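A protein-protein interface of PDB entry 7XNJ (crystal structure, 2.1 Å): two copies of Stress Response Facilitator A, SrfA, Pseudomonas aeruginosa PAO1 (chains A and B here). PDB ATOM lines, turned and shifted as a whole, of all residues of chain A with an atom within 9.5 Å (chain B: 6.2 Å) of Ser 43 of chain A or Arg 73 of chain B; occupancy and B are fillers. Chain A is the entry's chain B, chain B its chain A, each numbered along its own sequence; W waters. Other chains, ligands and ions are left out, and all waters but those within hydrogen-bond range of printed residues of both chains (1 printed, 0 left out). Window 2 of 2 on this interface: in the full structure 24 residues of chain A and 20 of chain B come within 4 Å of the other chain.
Of the printed residues of chain B, Tyr 42 of chain A touches Arg 73 (3.5 Å).
Of the printed residues of chain B, Arg 51 of chain A touches Ser 70 (3.7 Å).
Arg 11 of chain B touches none of the printed residues of chain A.
Printed residues of chain A within 4 Å of Leu 69 of chain B: Leu 37 (3.5 Å).
Printed residues of chain A within 4 Å of Ser 70 of chain B: Arg 51.
Arg 73 of chain B touches just these residues of chain A: Tyr 42 (3.5 Å), Ser 43 (2.9 Å) and Tyr 47 (3.98 Å).
The nearest printed residue of chain B that does not touch Ser 43 of chain A is Lys 7 of chain B (8.2 Å).
CD2 of Leu 37 of chain A touches CD1 of Leu 69 of chain B, 3.5 Å away.
Leu 37 of chain A touches Leu 72 of chain B.
Arg 38 of chain A touches Leu 72 of chain B.
CD2 of Tyr 47 of chain A touches NH2 of Arg 73 of chain B, at 3.98 Å.
NH2 of Arg 51 of chain A touches CB of Ser 70 of chain B (3.7 Å).
No position is printed for both chains.
Of the 8 pairs that touch across the chains among the printed residues, none has its exchanged pair printed and touching as well.
The guanidinium group of Arg 11 of chain B lies within hydrogen-bond range of the backbone carbonyl oxygen of Arg 73 of chain B (2.6 Å).
OG of Ser 40 of chain A sits at hydrogen-bond distance from N of Tyr 42 of chain A (3.1 Å).
Water W1 lies within hydrogen-bond range of O of Leu 69 of chain B (2.9 Å), N of Arg 73 of chain B (3.3 Å) and NH1 of Arg 51 of chain A (3.4 Å).
The guanidinium group of Arg 73 of chain B sits at hydrogen-bond distance from the backbone carbonyl oxygen of Tyr 42 of chain A (3.5 Å).
The guanidinium group of Arg 73 of chain B sits at hydrogen-bond distance from the side-chain hydroxyl of Ser 43 of chain A.
O of Leu 72 of chain B sits at hydrogen-bond distance from OH of Tyr 47 of chain A.
Of the 7 printed residues of chain B, 4 touch a printed residue of chain A.
Printed residues of chain B that touch a printed residue of chain A: Leu 69, Ser 70, Leu 72 and Arg 73.
Hydrophobic or aromatic side chains of chain B within 4 Å of the printed part of chain A: Leu 69 and Leu 72.
Hydrophobic or aromatic side chains of chain A within 4 Å of the printed part of chain B: Leu 37 and Tyr 47.
Along chain A the printed residues that touch a printed residue of chain B span positions 37 to 51.
Among the printed residues, no Asp or Glu carboxylate lies within 4 Å of a Lys or Arg side-chain nitrogen of the other chain.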
ATOM      1  N   LEU A  37      16.917  25.124  -4.201  1.00  0.00           N
ATOM      2  CA  LEU A  37      17.593  24.204  -3.301  1.00  0.00           C
ATOM      3  C   LEU A  37      17.083  24.349  -1.868  1.00  0.00           C
ATOM      4  O   LEU A  37      16.728  23.359  -1.220  1.00  0.00           O
ATOM      5  CB  LEU A  37      19.096  24.442  -3.363  1.00  0.00           C
ATOM      6  CG  LEU A  37      19.912  23.495  -2.499  1.00  0.00           C
ATOM      7  CD1 LEU A  37      20.023  22.129  -3.164  1.00  0.00           C
ATOM      8  CD2 LEU A  37      21.264  24.114  -2.263  1.00  0.00           C
ATOM      9  N   ARG A  38      17.054  25.579  -1.350  1.00  0.00           N
ATOM     10  CA  ARG A  38      16.553  25.806   0.003  1.00  0.00           C
ATOM     11  C   ARG A  38      15.138  25.262   0.171  1.00  0.00           C
ATOM     12  O   ARG A  38      14.777  24.764   1.241  1.00  0.00           O
ATOM     13  CB  ARG A  38      16.592  27.300   0.326  1.00  0.00           C
ATOM     14  CG  ARG A  38      16.070  27.654   1.720  1.00  0.00           C
ATOM     15  CD  ARG A  38      16.521  29.048   2.147  1.00  0.00           C
ATOM     16  NE  ARG A  38      15.717  29.583   3.244  1.00  0.00           N
ATOM     17  CZ  ARG A  38      15.910  29.286   4.521  1.00  0.00           C
ATOM     18  NH1 ARG A  38      16.857  28.440   4.898  1.00  0.00           N
ATOM     19  NH2 ARG A  38      15.145  29.863   5.444  1.00  0.00           N
ATOM     20  N   SER A  40      13.978  22.695  -1.358  1.00  0.00           N
ATOM     21  CA  SER A  40      13.947  21.339  -1.888  1.00  0.00           C
ATOM     22  C   SER A  40      13.858  20.320  -0.762  1.00  0.00           C
ATOM     23  O   SER A  40      14.575  20.425   0.237  1.00  0.00           O
ATOM     24  CB  SER A  40      15.186  21.049  -2.735  1.00  0.00           C
ATOM     25  OG  SER A  40      15.046  19.809  -3.399  1.00  0.00           O
ATOM     26  N   GLY A  41      12.991  19.331  -0.940  1.00  0.00           N
ATOM     27  CA  GLY A  41      12.959  18.167  -0.089  1.00  0.00           C
ATOM     28  C   GLY A  41      13.875  17.064  -0.557  1.00  0.00           C
ATOM     29  O   GLY A  41      13.849  15.966   0.012  1.00  0.00           O
ATOM     30  N   TYR A  42      14.684  17.324  -1.585  1.00  0.00           N
ATOM     31  CA  TYR A  42      15.612  16.326  -2.083  1.00  0.00           C
ATOM     32  C   TYR A  42      16.630  15.957  -1.007  1.00  0.00           C
ATOM     33  O   TYR A  42      16.735  16.592   0.052  1.00  0.00           O
ATOM     34  CB  TYR A  42      16.347  16.838  -3.320  1.00  0.00           C
ATOM     35  CG  TYR A  42      15.608  16.631  -4.622  1.00  0.00           C
ATOM     36  CD1 TYR A  42      14.894  15.464  -4.859  1.00  0.00           C
ATOM     37  CD2 TYR A  42      15.650  17.591  -5.628  1.00  0.00           C
ATOM     38  CE1 TYR A  42      14.222  15.263  -6.054  1.00  0.00           C
ATOM     39  CE2 TYR A  42      14.982  17.402  -6.823  1.00  0.00           C
ATOM     40  CZ  TYR A  42      14.271  16.232  -7.032  1.00  0.00           C
ATOM     41  OH  TYR A  42      13.609  16.031  -8.222  1.00  0.00           O
ATOM     42  N   SER A  43      17.394  14.904  -1.300  1.00  0.00           N
ATOM     43  CA  SER A  43      18.535  14.520  -0.488  1.00  0.00           C
ATOM     44  C   SER A  43      19.518  13.774  -1.376  1.00  0.00           C
ATOM     45  O   SER A  43      19.287  13.597  -2.576  1.00  0.00           O
ATOM     46  CB  SER A  43      18.108  13.677   0.710  1.00  0.00           C
ATOM     47  OG  SER A  43      19.212  13.456   1.563  1.00  0.00           O
ATOM     48  N   GLY A  44      20.632  13.358  -0.780  1.00  0.00           N
ATOM     49  CA  GLY A  44      21.603  12.543  -1.491  1.00  0.00           C
ATOM     50  C   GLY A  44      22.087  13.184  -2.776  1.00  0.00           C
ATOM     51  O   GLY A  44      22.418  14.374  -2.826  1.00  0.00           O
ATOM     52  N   ALA A  45      22.116  12.382  -3.841  1.00  0.00           N
ATOM     53  CA  ALA A  45      22.665  12.841  -5.109  1.00  0.00           C
ATOM     54  C   ALA A  45      21.804  13.918  -5.747  1.00  0.00           C
ATOM     55  O   ALA A  45      22.333  14.800  -6.436  1.00  0.00           O
ATOM     56  CB  ALA A  45      22.819  11.661  -6.067  1.00  0.00           C
ATOM     57  N   GLU A  46      20.490  13.871  -5.533  1.00  0.00           N
ATOM     58  CA  GLU A  46      19.629  14.854  -6.180  1.00  0.00           C
ATOM     59  C   GLU A  46      19.786  16.225  -5.543  1.00  0.00           C
ATOM     60  O   GLU A  46      19.819  17.238  -6.250  1.00  0.00           O
ATOM     61  CB  GLU A  46      18.170  14.422  -6.139  1.00  0.00           C
ATOM     62  CG  GLU A  46      17.437  14.863  -7.385  1.00  0.00           C
ATOM     63  CD  GLU A  46      17.398  13.790  -8.445  1.00  0.00           C
ATOM     64  OE1 GLU A  46      17.710  12.622  -8.118  1.00  0.00           O
ATOM     65  OE2 GLU A  46      17.085  14.124  -9.607  1.00  0.00           O
ATOM     66  N   TYR A  47      19.846  16.279  -4.212  1.00  0.00           N
ATOM     67  CA  TYR A  47      20.190  17.527  -3.548  1.00  0.00           C
ATOM     68  C   TYR A  47      21.524  18.051  -4.051  1.00  0.00           C
ATOM     69  O   TYR A  47      21.658  19.244  -4.344  1.00  0.00           O
ATOM     70  CB  TYR A  47      20.239  17.324  -2.040  1.00  0.00           C
ATOM     71  CG  TYR A  47      20.052  18.591  -1.246  1.00  0.00           C
ATOM     72  CD1 TYR A  47      21.137  19.385  -0.899  1.00  0.00           C
ATOM     73  CD2 TYR A  47      18.793  18.984  -0.835  1.00  0.00           C
ATOM     74  CE1 TYR A  47      20.963  20.549  -0.159  1.00  0.00           C
ATOM     75  CE2 TYR A  47      18.606  20.131  -0.105  1.00  0.00           C
ATOM     76  CZ  TYR A  47      19.692  20.910   0.233  1.00  0.00           C
ATOM     77  OH  TYR A  47      19.479  22.051   0.967  1.00  0.00           O
ATOM     78  N   ASP A  48      22.514  17.162  -4.173  1.00  0.00           N
ATOM     79  CA  ASP A  48      23.837  17.548  -4.650  1.00  0.00           C
ATOM     80  C   ASP A  48      23.765  18.186  -6.030  1.00  0.00           C
ATOM     81  O   ASP A  48      24.394  19.221  -6.281  1.00  0.00           O
ATOM     82  CB  ASP A  48      24.743  16.321  -4.692  1.00  0.00           C
ATOM     83  CG  ASP A  48      25.553  16.160  -3.437  1.00  0.00           C
ATOM     84  OD1 ASP A  48      26.435  17.015  -3.193  1.00  0.00           O
ATOM     85  OD2 ASP A  48      25.298  15.185  -2.695  1.00  0.00           O
ATOM     86  N   GLN A  49      23.020  17.565  -6.946  1.00  0.00           N
ATOM     87  CA  GLN A  49      22.974  18.063  -8.316  1.00  0.00           C
ATOM     88  C   GLN A  49      22.330  19.439  -8.374  1.00  0.00           C
ATOM     89  O   GLN A  49      22.832  20.330  -9.068  1.00  0.00           O
ATOM     90  CB  GLN A  49      22.237  17.070  -9.212  1.00  0.00           C
ATOM     91  CG  GLN A  49      22.981  15.742  -9.371  1.00  0.00           C
ATOM     92  CD  GLN A  49      22.208  14.708 -10.175  1.00  0.00           C
ATOM     93  OE1 GLN A  49      21.241  15.029 -10.867  1.00  0.00           O
ATOM     94  NE2 GLN A  49      22.622  13.450 -10.067  1.00  0.00           N
ATOM     95  N   LEU A  50      21.222  19.633  -7.654  1.00  0.00           N
ATOM     96  CA  LEU A  50      20.627  20.960  -7.563  1.00  0.00           C
ATOM     97  C   LEU A  50      21.607  21.955  -6.955  1.00  0.00           C
ATOM     98  O   LEU A  50      21.699  23.103  -7.399  1.00  0.00           O
ATOM     99  CB  LEU A  50      19.337  20.894  -6.745  1.00  0.00           C
ATOM    100  CG  LEU A  50      18.365  22.058  -6.922  1.00  0.00           C
ATOM    101  CD1 LEU A  50      18.025  22.229  -8.390  1.00  0.00           C
ATOM    102  CD2 LEU A  50      17.104  21.819  -6.096  1.00  0.00           C
ATOM    103  N   ARG A  51      22.365  21.519  -5.951  1.00  0.00           N
ATOM    104  CA  ARG A  51      23.350  22.383  -5.311  1.00  0.00           C
ATOM    105  C   ARG A  51      24.491  22.725  -6.261  1.00  0.00           C
ATOM    106  O   ARG A  51      24.904  23.887  -6.350  1.00  0.00           O
ATOM    107  CB  ARG A  51      23.871  21.701  -4.047  1.00  0.00           C
ATOM    108  CG  ARG A  51      24.803  22.514  -3.183  1.00  0.00           C
ATOM    109  CD  ARG A  51      25.592  21.583  -2.271  1.00  0.00           C
ATOM    110  NE  ARG A  51      26.945  22.066  -2.034  1.00  0.00           N
ATOM    111  CZ  ARG A  51      27.565  22.003  -0.863  1.00  0.00           C
ATOM    112  NH1 ARG A  51      26.984  21.468   0.198  1.00  0.00           N
ATOM    113  NH2 ARG A  51      28.794  22.508  -0.750  1.00  0.00           N
ATOM    114  N   LYS B   7      17.455  24.051   9.928  1.00  0.00           N
ATOM    115  CA  LYS B   7      18.763  23.531  10.325  1.00  0.00           C
ATOM    116  C   LYS B   7      19.929  24.481   9.976  1.00  0.00           C
ATOM    117  O   LYS B   7      21.006  24.408  10.582  1.00  0.00           O
ATOM    118  CB  LYS B   7      18.993  22.159   9.684  1.00  0.00           C
ATOM    119  CG  LYS B   7      18.433  20.998  10.497  1.00  0.00           C
ATOM    120  CD  LYS B   7      18.978  19.661  10.010  1.00  0.00           C
ATOM    121  CE  LYS B   7      18.439  19.327   8.622  1.00  0.00           C
ATOM    122  NZ  LYS B   7      18.227  17.862   8.424  1.00  0.00           N
ATOM    123  N   ARG B  11      24.643  26.546  12.278  1.00  0.00           N
ATOM    124  CA  ARG B  11      26.057  26.786  11.996  1.00  0.00           C
ATOM    125  C   ARG B  11      26.619  27.906  12.864  1.00  0.00           C
ATOM    126  O   ARG B  11      27.614  27.717  13.572  1.00  0.00           O
ATOM    127  CB  ARG B  11      26.251  27.097  10.507  1.00  0.00           C
ATOM    128  CG  ARG B  11      26.680  25.892   9.675  1.00  0.00           C
ATOM    129  CD  ARG B  11      25.926  24.656  10.121  1.00  0.00           C
ATOM    130  NE  ARG B  11      26.126  23.490   9.269  1.00  0.00           N
ATOM    131  CZ  ARG B  11      25.646  23.371   8.040  1.00  0.00           C
ATOM    132  NH1 ARG B  11      24.992  24.358   7.458  1.00  0.00           N
ATOM    133  NH2 ARG B  11      25.823  22.229   7.385  1.00  0.00           N
ATOM    134  N   LEU B  69      25.023  29.215   0.291  1.00  0.00           N
ATOM    135  CA  LEU B  69      24.619  28.032  -0.457  1.00  0.00           C
ATOM    136  C   LEU B  69      25.161  26.755   0.186  1.00  0.00           C
ATOM    137  O   LEU B  69      24.460  25.743   0.274  1.00  0.00           O
ATOM    138  CB  LEU B  69      25.100  28.151  -1.906  1.00  0.00           C
ATOM    139  CG  LEU B  69      25.173  26.844  -2.697  1.00  0.00           C
ATOM    140  CD1 LEU B  69      23.775  26.409  -3.087  1.00  0.00           C
ATOM    141  CD2 LEU B  69      26.050  26.942  -3.933  1.00  0.00           C
ATOM    142  N   SER B  70      26.412  26.776   0.635  1.00  0.00           N
ATOM    143  CA  SER B  70      26.982  25.533   1.147  1.00  0.00           C
ATOM    144  C   SER B  70      26.425  25.200   2.519  1.00  0.00           C
ATOM    145  O   SER B  70      26.319  24.021   2.871  1.00  0.00           O
ATOM    146  CB  SER B  70      28.506  25.608   1.190  1.00  0.00           C
ATOM    147  OG  SER B  70      28.919  26.353   2.318  1.00  0.00           O
ATOM    148  N   ASP B  71      26.033  26.217   3.288  1.00  0.00           N
ATOM    149  CA  ASP B  71      25.470  25.996   4.613  1.00  0.00           C
ATOM    150  C   ASP B  71      24.037  25.481   4.570  1.00  0.00           C
ATOM    151  O   ASP B  71      23.449  25.230   5.632  1.00  0.00           O
ATOM    152  CB  ASP B  71      25.531  27.284   5.430  1.00  0.00           C
ATOM    153  CG  ASP B  71      26.949  27.631   5.864  1.00  0.00           C
ATOM    154  OD1 ASP B  71      27.856  26.781   5.683  1.00  0.00           O
ATOM    155  OD2 ASP B  71      27.159  28.754   6.375  1.00  0.00           O
ATOM    156  N   LEU B  72      23.460  25.313   3.384  1.00  0.00           N
ATOM    157  CA  LEU B  72      22.102  24.795   3.300  1.00  0.00           C
ATOM    158  C   LEU B  72      22.005  23.305   3.610  1.00  0.00           C
ATOM    159  O   LEU B  72      20.922  22.836   3.977  1.00  0.00           O
ATOM    160  CB  LEU B  72      21.505  25.093   1.927  1.00  0.00           C
ATOM    161  CG  LEU B  72      21.026  26.541   1.829  1.00  0.00           C
ATOM    162  CD1 LEU B  72      20.560  26.877   0.423  1.00  0.00           C
ATOM    163  CD2 LEU B  72      19.919  26.776   2.829  1.00  0.00           C
ATOM    164  N   ARG B  73      23.088  22.545   3.495  1.00  0.00           N
ATOM    165  CA  ARG B  73      23.038  21.200   4.072  1.00  0.00           C
ATOM    166  C   ARG B  73      23.865  21.106   5.337  1.00  0.00           C
ATOM    167  O   ARG B  73      25.078  20.893   5.278  1.00  0.00           O
ATOM    168  CB  ARG B  73      23.510  20.137   3.092  1.00  0.00           C
ATOM    169  CG  ARG B  73      23.277  18.742   3.646  1.00  0.00           C
ATOM    170  CD  ARG B  73      21.798  18.508   3.958  1.00  0.00           C
ATOM    171  NE  ARG B  73      21.152  17.726   2.909  1.00  0.00           N
ATOM    172  CZ  ARG B  73      20.003  17.075   3.042  1.00  0.00           C
ATOM    173  NH1 ARG B  73      19.296  17.139   4.161  1.00  0.00           N
ATOM    174  NH2 ARG B  73      19.558  16.335   2.029  1.00  0.00           N
HETATM  175  O   HOH W   1      23.908  22.905   0.358  1.00  0.00           O
